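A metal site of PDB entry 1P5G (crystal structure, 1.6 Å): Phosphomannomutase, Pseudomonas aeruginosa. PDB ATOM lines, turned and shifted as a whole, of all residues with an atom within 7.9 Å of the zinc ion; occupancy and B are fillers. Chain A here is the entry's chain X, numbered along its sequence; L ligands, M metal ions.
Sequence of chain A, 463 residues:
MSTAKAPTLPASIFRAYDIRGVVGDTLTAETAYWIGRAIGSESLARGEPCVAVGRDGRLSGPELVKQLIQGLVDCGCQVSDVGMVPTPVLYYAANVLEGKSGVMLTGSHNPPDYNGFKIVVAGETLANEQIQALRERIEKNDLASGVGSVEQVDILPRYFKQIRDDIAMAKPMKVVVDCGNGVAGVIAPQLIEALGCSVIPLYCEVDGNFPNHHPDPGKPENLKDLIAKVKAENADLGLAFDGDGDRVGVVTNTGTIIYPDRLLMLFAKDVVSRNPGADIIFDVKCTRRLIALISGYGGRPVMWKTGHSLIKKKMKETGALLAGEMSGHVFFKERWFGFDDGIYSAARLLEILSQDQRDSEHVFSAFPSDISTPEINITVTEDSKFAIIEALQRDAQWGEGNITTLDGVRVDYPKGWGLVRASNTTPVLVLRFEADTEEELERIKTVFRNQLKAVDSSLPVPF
An oxygen (O3) of the ligand is in hydrogen-bond range of the backbone NH (N) of His 308.
A ring nitrogen (NE2) of His 329 lies within hydrogen-bond range of an oxygen (O2) of the ligand (3.0 Å).
An oxygen (O1) of the ligand sits at hydrogen-bond distance from O1P of SEP 108 (2.5 Å).
OG of Ser 327 is in hydrogen-bond range of O4 of the ligand (2.8 Å).
The side-chain carboxylate of Asp 246 is in salt-bridge range of the side-chain amino group of Lys 118 (2.7 Å).
The side-chain carboxylate (OD1) of Asp 244 sits at hydrogen-bond distance from the side-chain hydroxyl (OG1) of Thr 87.
O2P of SEP 108 lies within salt-bridge range of the side-chain amino group of Lys 118 (2.7 Å).
A ring nitrogen (ND1) of His 329 is in hydrogen-bond range of the backbone carbonyl oxygen (O) of Asp 246 (3.4 Å).
N of Gly 245 sits at hydrogen-bond distance from OD1 of Asp 242, at 3.0 Å.
O3P of SEP 108 lies close to a ring nitrogen (NE2) of His 329 (3.3 Å).
OG1 of Thr 106 lies within hydrogen-bond range of N of SEP 108.
NH1 of Arg 20 is in salt-bridge range of O2P of SEP 108 (3.0 Å).
Residues that only touch the zinc ion: Arg 247 (3.9 Å) and Lys 118 (3.9 Å).
Of the 25 residues printed, 6 come within 4 Å of the zinc ion.
The nearest printed residue that does not touch the zinc ion is His 329 (4.1 Å).
The zinc ion is bound by OD1 of Asp 246 (1.9 Å), OD2 of Asp 242 (2.0 Å), O3P of SEP 108 (2.0 Å) and OD2 of Asp 244 (2.0 Å).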
ATOM      1  N   ARG A  20     -12.465 -21.509  -3.754  1.00  0.00           N
ATOM      2  CA  ARG A  20     -13.819 -21.089  -3.376  1.00  0.00           C
ATOM      3  C   ARG A  20     -13.733 -20.084  -2.229  1.00  0.00           C
ATOM      4  O   ARG A  20     -13.004 -20.310  -1.259  1.00  0.00           O
ATOM      5  CB  ARG A  20     -14.644 -22.285  -2.919  1.00  0.00           C
ATOM      6  CG  ARG A  20     -16.126 -21.991  -2.637  1.00  0.00           C
ATOM      7  CD  ARG A  20     -17.054 -21.913  -3.877  1.00  0.00           C
ATOM      8  NE  ARG A  20     -16.828 -23.047  -4.770  1.00  0.00           N
ATOM      9  CZ  ARG A  20     -17.431 -24.225  -4.670  1.00  0.00           C
ATOM     10  NH1 ARG A  20     -17.127 -25.195  -5.524  1.00  0.00           N
ATOM     11  NH2 ARG A  20     -18.331 -24.459  -3.728  1.00  0.00           N
ATOM     12  N   ASP A  56     -20.645 -18.895 -14.355  1.00  0.00           N
ATOM     13  CA  ASP A  56     -22.007 -19.308 -14.100  1.00  0.00           C
ATOM     14  C   ASP A  56     -22.899 -18.063 -14.009  1.00  0.00           C
ATOM     15  O   ASP A  56     -22.512 -16.958 -14.483  1.00  0.00           O
ATOM     16  CB  ASP A  56     -22.090 -20.248 -12.886  1.00  0.00           C
ATOM     17  CG  ASP A  56     -21.770 -19.579 -11.576  1.00  0.00           C
ATOM     18  OD1 ASP A  56     -21.654 -18.343 -11.511  1.00  0.00           O
ATOM     19  OD2 ASP A  56     -21.658 -20.262 -10.532  1.00  0.00           O
ATOM     20  N   THR A  87     -20.818 -25.174 -15.946  1.00  0.00           N
ATOM     21  CA  THR A  87     -19.488 -25.759 -15.752  1.00  0.00           C
ATOM     22  C   THR A  87     -19.111 -26.834 -16.782  1.00  0.00           C
ATOM     23  O   THR A  87     -18.016 -26.738 -17.354  1.00  0.00           O
ATOM     24  CB  THR A  87     -19.401 -26.302 -14.321  1.00  0.00           C
ATOM     25  OG1 THR A  87     -19.348 -25.190 -13.430  1.00  0.00           O
ATOM     26  CG2 THR A  87     -18.126 -27.168 -14.070  1.00  0.00           C
ATOM     27  N   PRO A  88     -19.926 -27.866 -17.012  1.00  0.00           N
ATOM     28  CA  PRO A  88     -19.519 -28.868 -18.016  1.00  0.00           C
ATOM     29  C   PRO A  88     -19.331 -28.308 -19.411  1.00  0.00           C
ATOM     30  O   PRO A  88     -18.582 -28.895 -20.170  1.00  0.00           O
ATOM     31  CB  PRO A  88     -20.661 -29.898 -17.994  1.00  0.00           C
ATOM     32  CG  PRO A  88     -21.786 -29.226 -17.380  1.00  0.00           C
ATOM     33  CD  PRO A  88     -21.226 -28.222 -16.416  1.00  0.00           C
ATOM     34  N   TYR A  91     -15.892 -27.203 -19.421  1.00  0.00           N
ATOM     35  CA  TYR A  91     -15.039 -28.382 -19.559  1.00  0.00           C
ATOM     36  C   TYR A  91     -15.064 -28.886 -21.004  1.00  0.00           C
ATOM     37  O   TYR A  91     -14.051 -29.329 -21.555  1.00  0.00           O
ATOM     38  CB  TYR A  91     -15.456 -29.502 -18.620  1.00  0.00           C
ATOM     39  CG  TYR A  91     -15.358 -29.259 -17.138  1.00  0.00           C
ATOM     40  CD1 TYR A  91     -16.168 -29.977 -16.250  1.00  0.00           C
ATOM     41  CD2 TYR A  91     -14.475 -28.339 -16.585  1.00  0.00           C
ATOM     42  CE1 TYR A  91     -16.065 -29.806 -14.878  1.00  0.00           C
ATOM     43  CE2 TYR A  91     -14.387 -28.154 -15.217  1.00  0.00           C
ATOM     44  CZ  TYR A  91     -15.179 -28.894 -14.368  1.00  0.00           C
ATOM     45  OH  TYR A  91     -15.061 -28.725 -13.013  1.00  0.00           O
ATOM     46  N   THR A 106     -17.095 -20.203 -10.821  1.00  0.00           N
ATOM     47  CA  THR A 106     -18.319 -20.667 -10.203  1.00  0.00           C
ATOM     48  C   THR A 106     -18.204 -20.864  -8.698  1.00  0.00           C
ATOM     49  O   THR A 106     -17.133 -21.189  -8.166  1.00  0.00           O
ATOM     50  CB  THR A 106     -18.800 -21.979 -10.876  1.00  0.00           C
ATOM     51  OG1 THR A 106     -20.059 -22.386 -10.295  1.00  0.00           O
ATOM     52  CG2 THR A 106     -17.829 -23.135 -10.635  1.00  0.00           C
ATOM     53  N   GLY A 107     -19.326 -20.623  -8.031  1.00  0.00           N
ATOM     54  CA  GLY A 107     -19.534 -20.942  -6.632  1.00  0.00           C
ATOM     55  C   GLY A 107     -20.423 -22.161  -6.445  1.00  0.00           C
ATOM     56  O   GLY A 107     -20.911 -22.420  -5.344  1.00  0.00           O
ATOM     57  N   SEP A 108     -20.662 -22.906  -7.529  1.00  0.00           N
ATOM     58  CA  SEP A 108     -21.297 -24.202  -7.441  1.00  0.00           C
ATOM     59  CB  SEP A 108     -20.387 -25.175  -6.678  1.00  0.00           C
ATOM     60  OG  SEP A 108     -21.013 -26.422  -6.675  1.00  0.00           O
ATOM     61  C   SEP A 108     -22.719 -24.102  -6.876  1.00  0.00           C
ATOM     62  O   SEP A 108     -23.573 -23.477  -7.506  1.00  0.00           O
ATOM     63  P   SEP A 108     -20.125 -27.773  -6.569  1.00  0.00           P
ATOM     64  O1P SEP A 108     -20.524 -28.262  -5.103  1.00  0.00           O
ATOM     65  O2P SEP A 108     -18.549 -27.543  -6.695  1.00  0.00           O
ATOM     66  O3P SEP A 108     -20.657 -28.675  -7.732  1.00  0.00           O
ATOM     67  N   HIS A 109     -22.985 -24.721  -5.708  1.00  0.00           N
ATOM     68  CA  HIS A 109     -24.317 -24.749  -5.076  1.00  0.00           C
ATOM     69  C   HIS A 109     -24.414 -23.852  -3.837  1.00  0.00           C
ATOM     70  O   HIS A 109     -25.462 -23.843  -3.139  1.00  0.00           O
ATOM     71  CB  HIS A 109     -24.647 -26.167  -4.626  1.00  0.00           C
ATOM     72  CG  HIS A 109     -23.854 -26.609  -3.419  1.00  0.00           C
ATOM     73  ND1 HIS A 109     -22.768 -27.462  -3.514  1.00  0.00           N
ATOM     74  CD2 HIS A 109     -23.975 -26.309  -2.102  1.00  0.00           C
ATOM     75  CE1 HIS A 109     -22.273 -27.691  -2.310  1.00  0.00           C
ATOM     76  NE2 HIS A 109     -22.978 -26.992  -1.437  1.00  0.00           N
ATOM     77  N   ASN A 110     -23.347 -23.117  -3.549  1.00  0.00           N
ATOM     78  CA  ASN A 110     -23.246 -22.283  -2.352  1.00  0.00           C
ATOM     79  C   ASN A 110     -24.145 -21.056  -2.463  1.00  0.00           C
ATOM     80  O   ASN A 110     -24.631 -20.724  -3.557  1.00  0.00           O
ATOM     81  CB  ASN A 110     -21.793 -21.835  -2.127  1.00  0.00           C
ATOM     82  CG  ASN A 110     -20.910 -22.919  -1.537  1.00  0.00           C
ATOM     83  OD1 ASN A 110     -19.684 -22.848  -1.679  1.00  0.00           O
ATOM     84  ND2 ASN A 110     -21.492 -23.877  -0.841  1.00  0.00           N
ATOM     85  N   LYS A 118     -12.825 -23.426 -10.888  1.00  0.00           N
ATOM     86  CA  LYS A 118     -12.517 -24.818 -11.206  1.00  0.00           C
ATOM     87  C   LYS A 118     -11.570 -24.783 -12.394  1.00  0.00           C
ATOM     88  O   LYS A 118     -11.841 -24.084 -13.390  1.00  0.00           O
ATOM     89  CB  LYS A 118     -13.797 -25.580 -11.496  1.00  0.00           C
ATOM     90  CG  LYS A 118     -14.663 -25.706 -10.248  1.00  0.00           C
ATOM     91  CD  LYS A 118     -15.980 -26.393 -10.495  1.00  0.00           C
ATOM     92  CE  LYS A 118     -16.738 -26.597  -9.196  1.00  0.00           C
ATOM     93  NZ  LYS A 118     -17.965 -27.404  -9.364  1.00  0.00           N
ATOM     94  N   PRO A 215     -29.956 -23.891  -5.453  1.00  0.00           N
ATOM     95  CA  PRO A 215     -29.807 -24.965  -6.431  1.00  0.00           C
ATOM     96  C   PRO A 215     -28.836 -26.038  -5.891  1.00  0.00           C
ATOM     97  O   PRO A 215     -27.695 -26.089  -6.286  1.00  0.00           O
ATOM     98  CB  PRO A 215     -29.288 -24.245  -7.675  1.00  0.00           C
ATOM     99  CG  PRO A 215     -28.511 -23.093  -7.133  1.00  0.00           C
ATOM    100  CD  PRO A 215     -29.166 -22.696  -5.825  1.00  0.00           C
ATOM    101  N   PRO A 217     -29.460 -29.963  -5.155  1.00  0.00           N
ATOM    102  CA  PRO A 217     -30.328 -31.153  -5.173  1.00  0.00           C
ATOM    103  C   PRO A 217     -29.911 -32.291  -4.244  1.00  0.00           C
ATOM    104  O   PRO A 217     -30.572 -33.333  -4.250  1.00  0.00           O
ATOM    105  CB  PRO A 217     -30.248 -31.619  -6.636  1.00  0.00           C
ATOM    106  CG  PRO A 217     -29.003 -31.033  -7.178  1.00  0.00           C
ATOM    107  CD  PRO A 217     -28.709 -29.801  -6.410  1.00  0.00           C
ATOM    108  N   PHE A 241     -31.042 -29.701 -11.144  1.00  0.00           N
ATOM    109  CA  PHE A 241     -29.643 -29.389 -11.359  1.00  0.00           C
ATOM    110  C   PHE A 241     -29.093 -28.498 -10.255  1.00  0.00           C
ATOM    111  O   PHE A 241     -29.826 -27.693  -9.668  1.00  0.00           O
ATOM    112  CB  PHE A 241     -29.455 -28.731 -12.735  1.00  0.00           C
ATOM    113  CG  PHE A 241     -29.827 -29.639 -13.858  1.00  0.00           C
ATOM    114  CD1 PHE A 241     -28.990 -30.668 -14.226  1.00  0.00           C
ATOM    115  CD2 PHE A 241     -31.060 -29.540 -14.474  1.00  0.00           C
ATOM    116  CE1 PHE A 241     -29.337 -31.560 -15.227  1.00  0.00           C
ATOM    117  CE2 PHE A 241     -31.403 -30.431 -15.484  1.00  0.00           C
ATOM    118  CZ  PHE A 241     -30.548 -31.441 -15.863  1.00  0.00           C
ATOM    119  N   ASP A 242     -27.800 -28.614  -9.947  1.00  0.00           N
ATOM    120  CA  ASP A 242     -27.201 -27.656  -9.030  1.00  0.00           C
ATOM    121  C   ASP A 242     -26.874 -26.376  -9.801  1.00  0.00           C
ATOM    122  O   ASP A 242     -27.126 -26.287 -11.010  1.00  0.00           O
ATOM    123  CB  ASP A 242     -25.996 -28.245  -8.275  1.00  0.00           C
ATOM    124  CG  ASP A 242     -24.722 -28.249  -9.057  1.00  0.00           C
ATOM    125  OD1 ASP A 242     -24.762 -28.329 -10.299  1.00  0.00           O
ATOM    126  OD2 ASP A 242     -23.622 -28.272  -8.447  1.00  0.00           O
ATOM    127  N   GLY A 243     -26.338 -25.393  -9.090  1.00  0.00           N
ATOM    128  CA  GLY A 243     -26.209 -24.046  -9.633  1.00  0.00           C
ATOM    129  C   GLY A 243     -25.407 -23.969 -10.904  1.00  0.00           C
ATOM    130  O   GLY A 243     -25.722 -23.162 -11.777  1.00  0.00           O
ATOM    131  N   ASP A 244     -24.384 -24.811 -11.033  1.00  0.00           N
ATOM    132  CA  ASP A 244     -23.488 -24.720 -12.199  1.00  0.00           C
ATOM    133  C   ASP A 244     -23.648 -25.876 -13.195  1.00  0.00           C
ATOM    134  O   ASP A 244     -22.989 -25.914 -14.228  1.00  0.00           O
ATOM    135  CB  ASP A 244     -22.014 -24.533 -11.773  1.00  0.00           C
ATOM    136  CG  ASP A 244     -21.486 -25.661 -10.929  1.00  0.00           C
ATOM    137  OD1 ASP A 244     -20.267 -25.937 -10.952  1.00  0.00           O
ATOM    138  OD2 ASP A 244     -22.227 -26.318 -10.165  1.00  0.00           O
ATOM    139  N   GLY A 245     -24.515 -26.836 -12.887  1.00  0.00           N
ATOM    140  CA  GLY A 245     -24.896 -27.886 -13.810  1.00  0.00           C
ATOM    141  C   GLY A 245     -23.997 -29.108 -13.905  1.00  0.00           C
ATOM    142  O   GLY A 245     -24.174 -29.919 -14.812  1.00  0.00           O
ATOM    143  N   ASP A 246     -23.051 -29.250 -12.975  1.00  0.00           N
ATOM    144  CA  ASP A 246     -22.234 -30.456 -12.946  1.00  0.00           C
ATOM    145  C   ASP A 246     -22.781 -31.546 -12.032  1.00  0.00           C
ATOM    146  O   ASP A 246     -22.182 -32.625 -11.925  1.00  0.00           O
ATOM    147  CB  ASP A 246     -20.770 -30.140 -12.632  1.00  0.00           C
ATOM    148  CG  ASP A 246     -20.566 -29.441 -11.342  1.00  0.00           C
ATOM    149  OD1 ASP A 246     -21.539 -29.261 -10.561  1.00  0.00           O
ATOM    150  OD2 ASP A 246     -19.439 -29.043 -11.005  1.00  0.00           O
ATOM    151  N   ARG A 247     -23.897 -31.269 -11.367  1.00  0.00           N
ATOM    152  CA  ARG A 247     -24.582 -32.264 -10.545  1.00  0.00           C
ATOM    153  C   ARG A 247     -26.035 -32.339 -10.930  1.00  0.00           C
ATOM    154  O   ARG A 247     -26.654 -31.318 -11.274  1.00  0.00           O
ATOM    155  CB  ARG A 247     -24.511 -31.901  -9.074  1.00  0.00           C
ATOM    156  CG  ARG A 247     -23.118 -31.948  -8.483  1.00  0.00           C
ATOM    157  CD  ARG A 247     -22.938 -31.156  -7.207  1.00  0.00           C
ATOM    158  NE  ARG A 247     -24.162 -30.859  -6.472  1.00  0.00           N
ATOM    159  CZ  ARG A 247     -24.286 -29.841  -5.636  1.00  0.00           C
ATOM    160  NH1 ARG A 247     -23.265 -29.035  -5.453  1.00  0.00           N
ATOM    161  NH2 ARG A 247     -25.415 -29.624  -4.966  1.00  0.00           N
ATOM    162  N   VAL A 248     -26.594 -33.546 -10.839  1.00  0.00           N
ATOM    163  CA  VAL A 248     -27.986 -33.794 -11.155  1.00  0.00           C
ATOM    164  C   VAL A 248     -28.601 -34.602  -9.998  1.00  0.00           C
ATOM    165  O   VAL A 248     -27.905 -35.382  -9.328  1.00  0.00           O
ATOM    166  CB  VAL A 248     -28.082 -34.572 -12.505  1.00  0.00           C
ATOM    167  CG1 VAL A 248     -27.423 -35.963 -12.431  1.00  0.00           C
ATOM    168  CG2 VAL A 248     -29.512 -34.670 -12.962  1.00  0.00           C
ATOM    169  N   HIS A 308     -14.586 -33.945  -7.064  1.00  0.00           N
ATOM    170  CA  HIS A 308     -14.634 -34.032  -8.529  1.00  0.00           C
ATOM    171  C   HIS A 308     -13.262 -34.100  -9.164  1.00  0.00           C
ATOM    172  O   HIS A 308     -13.006 -34.955 -10.015  1.00  0.00           O
ATOM    173  CB  HIS A 308     -15.507 -32.890  -9.116  1.00  0.00           C
ATOM    174  CG  HIS A 308     -14.896 -31.537  -9.007  1.00  0.00           C
ATOM    175  ND1 HIS A 308     -14.091 -31.007  -9.997  1.00  0.00           N
ATOM    176  CD2 HIS A 308     -14.951 -30.601  -8.027  1.00  0.00           C
ATOM    177  CE1 HIS A 308     -13.681 -29.800  -9.635  1.00  0.00           C
ATOM    178  NE2 HIS A 308     -14.192 -29.534  -8.446  1.00  0.00           N
ATOM    179  N   SER A 327     -22.391 -37.206  -4.177  1.00  0.00           N
ATOM    180  CA  SER A 327     -22.880 -35.827  -4.327  1.00  0.00           C
ATOM    181  C   SER A 327     -23.600 -35.527  -5.629  1.00  0.00           C
ATOM    182  O   SER A 327     -24.152 -34.452  -5.773  1.00  0.00           O
ATOM    183  CB  SER A 327     -21.755 -34.825  -4.153  1.00  0.00           C
ATOM    184  OG  SER A 327     -20.737 -35.078  -5.104  1.00  0.00           O
ATOM    185  N   HIS A 329     -22.196 -35.781  -8.873  1.00  0.00           N
ATOM    186  CA  HIS A 329     -21.286 -35.602  -9.995  1.00  0.00           C
ATOM    187  C   HIS A 329     -21.148 -36.962 -10.670  1.00  0.00           C
ATOM    188  O   HIS A 329     -20.754 -37.939 -10.014  1.00  0.00           O
ATOM    189  CB  HIS A 329     -19.895 -35.084  -9.542  1.00  0.00           C
ATOM    190  CG  HIS A 329     -19.908 -33.711  -8.946  1.00  0.00           C
ATOM    191  ND1 HIS A 329     -19.601 -32.583  -9.676  1.00  0.00           N
ATOM    192  CD2 HIS A 329     -20.153 -33.289  -7.689  1.00  0.00           C
ATOM    193  CE1 HIS A 329     -19.711 -31.519  -8.903  1.00  0.00           C
ATOM    194  NE2 HIS A 329     -20.044 -31.909  -7.687  1.00  0.00           N
ATOM    195  N   ASP A 340     -17.343 -34.462 -15.356  1.00  0.00           N
ATOM    196  CA  ASP A 340     -18.647 -34.442 -14.671  1.00  0.00           C
ATOM    197  C   ASP A 340     -19.594 -33.476 -15.363  1.00  0.00           C
ATOM    198  O   ASP A 340     -19.227 -32.365 -15.734  1.00  0.00           O
ATOM    199  CB  ASP A 340     -18.578 -34.144 -13.147  1.00  0.00           C
ATOM    200  CG  ASP A 340     -17.587 -33.041 -12.780  1.00  0.00           C
ATOM    201  OD1 ASP A 340     -17.855 -32.355 -11.756  1.00  0.00           O
ATOM    202  OD2 ASP A 340     -16.509 -32.869 -13.399  1.00  0.00           O
HETATM  203  C1  LIG L   1     -18.372 -30.450  -3.816  1.00  0.00           C
HETATM  204  C2  LIG L   1     -17.547 -31.129  -4.889  1.00  0.00           C
HETATM  205  C3  LIG L   1     -17.928 -32.613  -4.974  1.00  0.00           C
HETATM  206  C4  LIG L   1     -17.859 -33.263  -3.570  1.00  0.00           C
HETATM  207  C5  LIG L   1     -18.669 -32.440  -2.541  1.00  0.00           C
HETATM  208  C6  LIG L   1     -18.536 -32.996  -1.126  1.00  0.00           C
HETATM  209  O1  LIG L   1     -19.753 -30.487  -4.199  1.00  0.00           O
HETATM  210  O2  LIG L   1     -17.797 -30.523  -6.199  1.00  0.00           O
HETATM  211  O3  LIG L   1     -17.053 -33.211  -5.904  1.00  0.00           O
HETATM  212  O4  LIG L   1     -18.395 -34.543  -3.669  1.00  0.00           O
HETATM  213  O5  LIG L   1     -18.206 -31.109  -2.516  1.00  0.00           O
HETATM  214  O6  LIG L   1     -17.144 -32.865  -0.733  1.00  0.00           O
HETATM  215  P1  LIG L   1     -16.789 -33.106   0.795  1.00  0.00           P
HETATM  216  O7  LIG L   1     -17.447 -34.363   1.285  1.00  0.00           O
HETATM  217  O8  LIG L   1     -17.277 -31.929   1.591  1.00  0.00           O
HETATM  218  O9  LIG L   1     -15.282 -33.177   0.815  1.00  0.00           O
HETATM  219 ZN    ZN M   1     -21.827 -27.980  -9.153  1.00  0.00          ZN
